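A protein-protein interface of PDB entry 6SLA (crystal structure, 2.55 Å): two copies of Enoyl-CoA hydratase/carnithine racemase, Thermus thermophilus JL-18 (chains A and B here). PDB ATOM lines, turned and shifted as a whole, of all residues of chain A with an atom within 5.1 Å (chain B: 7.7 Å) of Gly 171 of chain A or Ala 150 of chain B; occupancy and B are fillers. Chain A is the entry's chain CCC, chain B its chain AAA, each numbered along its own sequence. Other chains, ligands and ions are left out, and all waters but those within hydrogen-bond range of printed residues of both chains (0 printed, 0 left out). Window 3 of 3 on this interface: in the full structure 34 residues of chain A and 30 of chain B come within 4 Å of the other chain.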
ATOM      1  N   ARG A 116     -23.809   5.597  -5.827  1.00  0.00           N
ATOM      2  CA  ARG A 116     -23.448   6.141  -7.118  1.00  0.00           C
ATOM      3  C   ARG A 116     -22.075   5.651  -7.551  1.00  0.00           C
ATOM      4  O   ARG A 116     -21.117   5.713  -6.787  1.00  0.00           O
ATOM      5  CB  ARG A 116     -23.559   7.665  -7.075  1.00  0.00           C
ATOM      6  CG  ARG A 116     -24.947   8.181  -6.710  1.00  0.00           C
ATOM      7  CD  ARG A 116     -25.074   9.667  -6.623  1.00  0.00           C
ATOM      8  NE  ARG A 116     -24.141  10.210  -5.642  1.00  0.00           N
ATOM      9  CZ  ARG A 116     -24.284  10.163  -4.322  1.00  0.00           C
ATOM     10  NH1 ARG A 116     -25.310   9.546  -3.779  1.00  0.00           N
ATOM     11  NH2 ARG A 116     -23.349  10.685  -3.548  1.00  0.00           N
ATOM     12  N   ARG A 145     -25.515  19.220   0.512  1.00  0.00           N
ATOM     13  CA  ARG A 145     -25.624  18.074   1.414  1.00  0.00           C
ATOM     14  C   ARG A 145     -24.557  17.020   1.083  1.00  0.00           C
ATOM     15  O   ARG A 145     -23.978  16.418   1.966  1.00  0.00           O
ATOM     16  CB  ARG A 145     -27.037  17.463   1.392  1.00  0.00           C
ATOM     17  CG  ARG A 145     -28.118  18.415   1.893  1.00  0.00           C
ATOM     18  CD  ARG A 145     -29.513  17.958   1.559  1.00  0.00           C
ATOM     19  NE  ARG A 145     -30.557  18.572   2.365  1.00  0.00           N
ATOM     20  CZ  ARG A 145     -30.976  19.815   2.230  1.00  0.00           C
ATOM     21  NH1 ARG A 145     -30.406  20.620   1.341  1.00  0.00           N
ATOM     22  NH2 ARG A 145     -31.938  20.260   3.017  1.00  0.00           N
ATOM     23  N   LEU A 146     -24.313  16.771  -0.203  1.00  0.00           N
ATOM     24  CA  LEU A 146     -23.452  15.680  -0.615  1.00  0.00           C
ATOM     25  C   LEU A 146     -21.972  16.020  -0.418  1.00  0.00           C
ATOM     26  O   LEU A 146     -21.201  15.162   0.024  1.00  0.00           O
ATOM     27  CB  LEU A 146     -23.749  15.322  -2.077  1.00  0.00           C
ATOM     28  CG  LEU A 146     -25.035  14.529  -2.319  1.00  0.00           C
ATOM     29  CD1 LEU A 146     -25.239  14.290  -3.803  1.00  0.00           C
ATOM     30  CD2 LEU A 146     -25.058  13.222  -1.546  1.00  0.00           C
ATOM     31  N   VAL A 147     -21.561  17.256  -0.759  1.00  0.00           N
ATOM     32  CA  VAL A 147     -20.129  17.525  -0.828  1.00  0.00           C
ATOM     33  C   VAL A 147     -19.746  18.662   0.109  1.00  0.00           C
ATOM     34  O   VAL A 147     -18.569  19.010   0.168  1.00  0.00           O
ATOM     35  CB  VAL A 147     -19.644  17.802  -2.263  1.00  0.00           C
ATOM     36  CG1 VAL A 147     -19.877  16.603  -3.165  1.00  0.00           C
ATOM     37  CG2 VAL A 147     -20.276  19.053  -2.854  1.00  0.00           C
ATOM     38  N   ALA A 167     -14.605  13.479  -8.590  1.00  0.00           N
ATOM     39  CA  ALA A 167     -15.965  13.278  -8.119  1.00  0.00           C
ATOM     40  C   ALA A 167     -15.991  12.289  -6.952  1.00  0.00           C
ATOM     41  O   ALA A 167     -16.731  12.498  -5.986  1.00  0.00           O
ATOM     42  CB  ALA A 167     -16.854  12.838  -9.252  1.00  0.00           C
ATOM     43  N   LEU A 168     -15.150  11.240  -7.037  1.00  0.00           N
ATOM     44  CA  LEU A 168     -15.006  10.258  -5.967  1.00  0.00           C
ATOM     45  C   LEU A 168     -14.483  10.931  -4.699  1.00  0.00           C
ATOM     46  O   LEU A 168     -14.989  10.686  -3.610  1.00  0.00           O
ATOM     47  CB  LEU A 168     -14.071   9.128  -6.410  1.00  0.00           C
ATOM     48  CG  LEU A 168     -13.743   8.058  -5.368  1.00  0.00           C
ATOM     49  CD1 LEU A 168     -14.988   7.236  -5.016  1.00  0.00           C
ATOM     50  CD2 LEU A 168     -12.610   7.167  -5.883  1.00  0.00           C
ATOM     51  N   ALA A 169     -13.480  11.797  -4.844  1.00  0.00           N
ATOM     52  CA  ALA A 169     -12.860  12.441  -3.698  1.00  0.00           C
ATOM     53  C   ALA A 169     -13.866  13.357  -2.998  1.00  0.00           C
ATOM     54  O   ALA A 169     -13.851  13.425  -1.781  1.00  0.00           O
ATOM     55  CB  ALA A 169     -11.621  13.192  -4.136  1.00  0.00           C
ATOM     56  N   LEU A 170     -14.759  14.016  -3.753  1.00  0.00           N
ATOM     57  CA  LEU A 170     -15.725  14.937  -3.184  1.00  0.00           C
ATOM     58  C   LEU A 170     -16.939  14.204  -2.597  1.00  0.00           C
ATOM     59  O   LEU A 170     -17.745  14.821  -1.906  1.00  0.00           O
ATOM     60  CB  LEU A 170     -16.221  15.900  -4.266  1.00  0.00           C
ATOM     61  CG  LEU A 170     -15.179  16.739  -4.988  1.00  0.00           C
ATOM     62  CD1 LEU A 170     -15.852  17.578  -6.038  1.00  0.00           C
ATOM     63  CD2 LEU A 170     -14.396  17.612  -3.999  1.00  0.00           C
ATOM     64  N   GLY A 171     -17.125  12.921  -2.922  1.00  0.00           N
ATOM     65  CA  GLY A 171     -18.336  12.216  -2.524  1.00  0.00           C
ATOM     66  C   GLY A 171     -19.472  12.271  -3.556  1.00  0.00           C
ATOM     67  O   GLY A 171     -20.549  11.731  -3.316  1.00  0.00           O
ATOM     68  N   LEU A 172     -19.241  12.903  -4.717  1.00  0.00           N
ATOM     69  CA  LEU A 172     -20.233  12.877  -5.790  1.00  0.00           C
ATOM     70  C   LEU A 172     -20.552  11.440  -6.213  1.00  0.00           C
ATOM     71  O   LEU A 172     -21.675  11.131  -6.614  1.00  0.00           O
ATOM     72  CB  LEU A 172     -19.720  13.686  -6.985  1.00  0.00           C
ATOM     73  CG  LEU A 172     -19.740  15.204  -6.840  1.00  0.00           C
ATOM     74  CD1 LEU A 172     -19.159  15.861  -8.085  1.00  0.00           C
ATOM     75  CD2 LEU A 172     -21.141  15.700  -6.562  1.00  0.00           C
ATOM     76  N   VAL A 173     -19.541  10.568  -6.177  1.00  0.00           N
ATOM     77  CA  VAL A 173     -19.771   9.158  -6.443  1.00  0.00           C
ATOM     78  C   VAL A 173     -19.090   8.371  -5.329  1.00  0.00           C
ATOM     79  O   VAL A 173     -18.200   8.891  -4.659  1.00  0.00           O
ATOM     80  CB  VAL A 173     -19.298   8.725  -7.848  1.00  0.00           C
ATOM     81  CG1 VAL A 173     -19.964   9.492  -8.969  1.00  0.00           C
ATOM     82  CG2 VAL A 173     -17.793   8.727  -8.012  1.00  0.00           C
ATOM     83  N   HIS A 174     -19.539   7.135  -5.136  1.00  0.00           N
ATOM     84  CA  HIS A 174     -19.056   6.297  -4.051  1.00  0.00           C
ATOM     85  C   HIS A 174     -17.976   5.339  -4.557  1.00  0.00           C
ATOM     86  O   HIS A 174     -17.199   4.834  -3.759  1.00  0.00           O
ATOM     87  CB  HIS A 174     -20.203   5.504  -3.417  1.00  0.00           C
ATOM     88  CG  HIS A 174     -21.283   6.341  -2.799  1.00  0.00           C
ATOM     89  ND1 HIS A 174     -22.510   6.566  -3.423  1.00  0.00           N
ATOM     90  CD2 HIS A 174     -21.363   6.960  -1.594  1.00  0.00           C
ATOM     91  CE1 HIS A 174     -23.276   7.292  -2.631  1.00  0.00           C
ATOM     92  NE2 HIS A 174     -22.595   7.552  -1.507  1.00  0.00           N
ATOM     93  N   PRO B 144     -25.243  12.615   8.991  1.00  0.00           N
ATOM     94  CA  PRO B 144     -25.153  13.449   7.789  1.00  0.00           C
ATOM     95  C   PRO B 144     -24.518  14.796   8.120  1.00  0.00           C
ATOM     96  O   PRO B 144     -23.781  15.329   7.299  1.00  0.00           O
ATOM     97  CB  PRO B 144     -26.589  13.627   7.302  1.00  0.00           C
ATOM     98  CG  PRO B 144     -27.368  12.560   8.065  1.00  0.00           C
ATOM     99  CD  PRO B 144     -26.636  12.295   9.355  1.00  0.00           C
ATOM    100  N   VAL B 147     -20.474  13.924   8.630  1.00  0.00           N
ATOM    101  CA  VAL B 147     -19.614  13.415   7.573  1.00  0.00           C
ATOM    102  C   VAL B 147     -20.170  13.742   6.196  1.00  0.00           C
ATOM    103  O   VAL B 147     -19.536  13.406   5.194  1.00  0.00           O
ATOM    104  CB  VAL B 147     -19.333  11.911   7.707  1.00  0.00           C
ATOM    105  CG1 VAL B 147     -18.526  11.599   8.950  1.00  0.00           C
ATOM    106  CG2 VAL B 147     -20.602  11.089   7.586  1.00  0.00           C
ATOM    107  N   GLY B 148     -21.350  14.381   6.172  1.00  0.00           N
ATOM    108  CA  GLY B 148     -22.011  14.792   4.950  1.00  0.00           C
ATOM    109  C   GLY B 148     -22.929  13.684   4.450  1.00  0.00           C
ATOM    110  O   GLY B 148     -22.745  12.504   4.828  1.00  0.00           O
ATOM    111  N   LEU B 149     -23.894  14.058   3.593  1.00  0.00           N
ATOM    112  CA  LEU B 149     -24.875  13.088   3.122  1.00  0.00           C
ATOM    113  C   LEU B 149     -24.251  11.911   2.369  1.00  0.00           C
ATOM    114  O   LEU B 149     -24.716  10.796   2.549  1.00  0.00           O
ATOM    115  CB  LEU B 149     -25.926  13.778   2.243  1.00  0.00           C
ATOM    116  CG  LEU B 149     -27.075  12.885   1.792  1.00  0.00           C
ATOM    117  CD1 LEU B 149     -27.812  12.417   3.020  1.00  0.00           C
ATOM    118  CD2 LEU B 149     -28.000  13.584   0.803  1.00  0.00           C
ATOM    119  N   ALA B 150     -23.232  12.151   1.542  1.00  0.00           N
ATOM    120  CA  ALA B 150     -22.695  11.095   0.675  1.00  0.00           C
ATOM    121  C   ALA B 150     -22.136   9.944   1.502  1.00  0.00           C
ATOM    122  O   ALA B 150     -22.468   8.798   1.218  1.00  0.00           O
ATOM    123  CB  ALA B 150     -21.718  11.575  -0.375  1.00  0.00           C
ATOM    124  N   LYS B 151     -21.346  10.244   2.538  1.00  0.00           N
ATOM    125  CA  LYS B 151     -20.771   9.216   3.395  1.00  0.00           C
ATOM    126  C   LYS B 151     -21.844   8.609   4.300  1.00  0.00           C
ATOM    127  O   LYS B 151     -21.780   7.411   4.607  1.00  0.00           O
ATOM    128  CB  LYS B 151     -19.606   9.752   4.233  1.00  0.00           C
ATOM    129  CG  LYS B 151     -18.183   9.573   3.725  1.00  0.00           C
ATOM    130  CD  LYS B 151     -17.795   8.116   3.607  1.00  0.00           C
ATOM    131  CE  LYS B 151     -16.677   7.878   2.606  1.00  0.00           C
ATOM    132  NZ  LYS B 151     -16.541   6.434   2.312  1.00  0.00           N
ATOM    133  N   ALA B 152     -22.823   9.435   4.708  1.00  0.00           N
ATOM    134  CA  ALA B 152     -23.913   8.950   5.540  1.00  0.00           C
ATOM    135  C   ALA B 152     -24.671   7.840   4.837  1.00  0.00           C
ATOM    136  O   ALA B 152     -24.877   6.784   5.438  1.00  0.00           O
ATOM    137  CB  ALA B 152     -24.826  10.068   5.966  1.00  0.00           C
ATOM    138  N   GLN B 153     -25.042   8.064   3.572  1.00  0.00           N
ATOM    139  CA  GLN B 153     -25.763   7.094   2.726  1.00  0.00           C
ATOM    140  C   GLN B 153     -25.014   5.769   2.723  1.00  0.00           C
ATOM    141  O   GLN B 153     -25.594   4.735   2.986  1.00  0.00           O
ATOM    142  CB  GLN B 153     -25.775   7.556   1.271  1.00  0.00           C
ATOM    143  CG  GLN B 153     -26.897   8.523   0.924  1.00  0.00           C
ATOM    144  CD  GLN B 153     -26.610   9.210  -0.395  1.00  0.00           C
ATOM    145  OE1 GLN B 153     -25.465   9.312  -0.843  1.00  0.00           O
ATOM    146  NE2 GLN B 153     -27.671   9.620  -1.076  1.00  0.00           N
ATOM    147  N   GLU B 154     -23.713   5.808   2.427  1.00  0.00           N
ATOM    148  CA  GLU B 154     -22.912   4.599   2.317  1.00  0.00           C
ATOM    149  C   GLU B 154     -22.803   3.934   3.691  1.00  0.00           C
ATOM    150  O   GLU B 154     -23.059   2.748   3.812  1.00  0.00           O
ATOM    151  CB  GLU B 154     -21.557   4.944   1.700  1.00  0.00           C
ATOM    152  CG  GLU B 154     -20.621   3.778   1.488  1.00  0.00           C
ATOM    153  CD  GLU B 154     -19.233   4.211   1.015  1.00  0.00           C
ATOM    154  OE1 GLU B 154     -19.012   5.450   0.856  1.00  0.00           O
ATOM    155  OE2 GLU B 154     -18.355   3.315   0.795  1.00  0.00           O
ATOM    156  N   LEU B 155     -22.469   4.704   4.733  1.00  0.00           N
ATOM    157  CA  LEU B 155     -22.241   4.117   6.041  1.00  0.00           C
ATOM    158  C   LEU B 155     -23.520   3.464   6.554  1.00  0.00           C
ATOM    159  O   LEU B 155     -23.455   2.386   7.157  1.00  0.00           O
ATOM    160  CB  LEU B 155     -21.755   5.190   7.024  1.00  0.00           C
ATOM    161  CG  LEU B 155     -20.320   5.693   6.842  1.00  0.00           C
ATOM    162  CD1 LEU B 155     -19.935   6.656   7.960  1.00  0.00           C
ATOM    163  CD2 LEU B 155     -19.319   4.560   6.747  1.00  0.00           C
ATOM    164  N   LEU B 156     -24.668   4.126   6.315  1.00  0.00           N
ATOM    165  CA  LEU B 156     -25.947   3.632   6.817  1.00  0.00           C
ATOM    166  C   LEU B 156     -26.482   2.461   5.983  1.00  0.00           C
ATOM    167  O   LEU B 156     -26.934   1.460   6.552  1.00  0.00           O
ATOM    168  CB  LEU B 156     -26.955   4.782   6.886  1.00  0.00           C
ATOM    169  CG  LEU B 156     -26.684   5.767   8.012  1.00  0.00           C
ATOM    170  CD1 LEU B 156     -27.610   6.983   7.896  1.00  0.00           C
ATOM    171  CD2 LEU B 156     -26.863   5.095   9.356  1.00  0.00           C
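The backbone NH (N) of Leu 149 of chain B sits at hydrogen-bond distance from the backbone carbonyl oxygen (O) of Arg 145 of chain A (2.9 Å).
The side-chain amide oxygen of Gln 153 of chain B sits at hydrogen-bond distance from a ring nitrogen (NE2) of His 174 of chain A (3.4 Å).
The backbone carbonyl oxygen (O) of Ala 150 of chain B lies within hydrogen-bond range of a ring nitrogen (NE2) of His 174 of chain A, 3.0 Å away.
The side-chain amide oxygen of Gln 153 of chain B is in hydrogen-bond range of the guanidinium group of Arg 116 of chain A (2.9 Å).
O of Arg 116 of chain A sits at hydrogen-bond distance from N of His 174 of chain A (2.7 Å).
The side-chain carboxylate (OE1) of Glu 154 of chain B lies within salt-bridge range of the side-chain amino group (NZ) of Lys 151 of chain B (3.0 Å).
The guanidinium group of Arg 116 of chain A is in hydrogen-bond range of the backbone carbonyl oxygen of Gly 171 of chain A, at 3.0 Å.
The backbone carbonyl oxygen (O) of Leu 172 of chain A lies within hydrogen-bond range of the guanidinium group (NE) of Arg 116 of chain A.
Among the printed residues, pairs that only touch across the chains: Gly 171 of chain A with Ala 150 of chain B, Leu 146 of chain A with Ala 150 of chain B, Arg 116 of chain A with Ala 150 of chain B, His 174 of chain A with Glu 154 of chain B, Leu 146 of chain A with Leu 149 of chain B, Arg 145 of chain A with Gly 148 of chain B and Leu 146 of chain A with Gln 153 of chain B.
Of the printed residues of chain B, Arg 116 of chain A touches Ala 150 (3.7 Å) and Gln 153 (2.9 Å).
Gly 171 of chain A touches just one residue of chain B: Ala 150.
Of the printed residues of chain B, His 174 of chain A touches Ala 150, Gln 153 and Glu 154.
Of the printed residues of chain A, Gly 148 of chain B touches Arg 145 (3.8 Å).
Of the printed residues of chain A, Leu 149 of chain B touches Arg 145 (2.9 Å) and Leu 146 (3.8 Å).
Ala 150 of chain B touches four residues of chain A.
Printed residues of chain A within 4 Å of Glu 154 of chain B: His 174 (3.7 Å).
The nearest residue of chain B that does not touch Gly 171 of chain A is Gln 153 of chain B (6.0 Å).
The nearest residue of chain A that does not touch Ala 150 of chain B is Arg 145 of chain A (4.4 Å).
The nearest printed residue of chain A that does not touch Gln 153 of chain B is Gly 171 of chain A (6.0 Å).
Hydrophobic or aromatic side chains of chain B that line the printed part of chain A: Leu 149 and Ala 150.
Of the 12 printed residues of chain A, 5 touch a printed residue of chain B.
Hydrophobic or aromatic side chains of chain A within 4 Å of the printed part of chain B: Leu 146 and His 174.
Among the printed residues, no Asp or Glu carboxylate lies within 4 Å of a Lys or Arg side-chain nitrogen of the other chain.
Position printed for both chains: 147.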
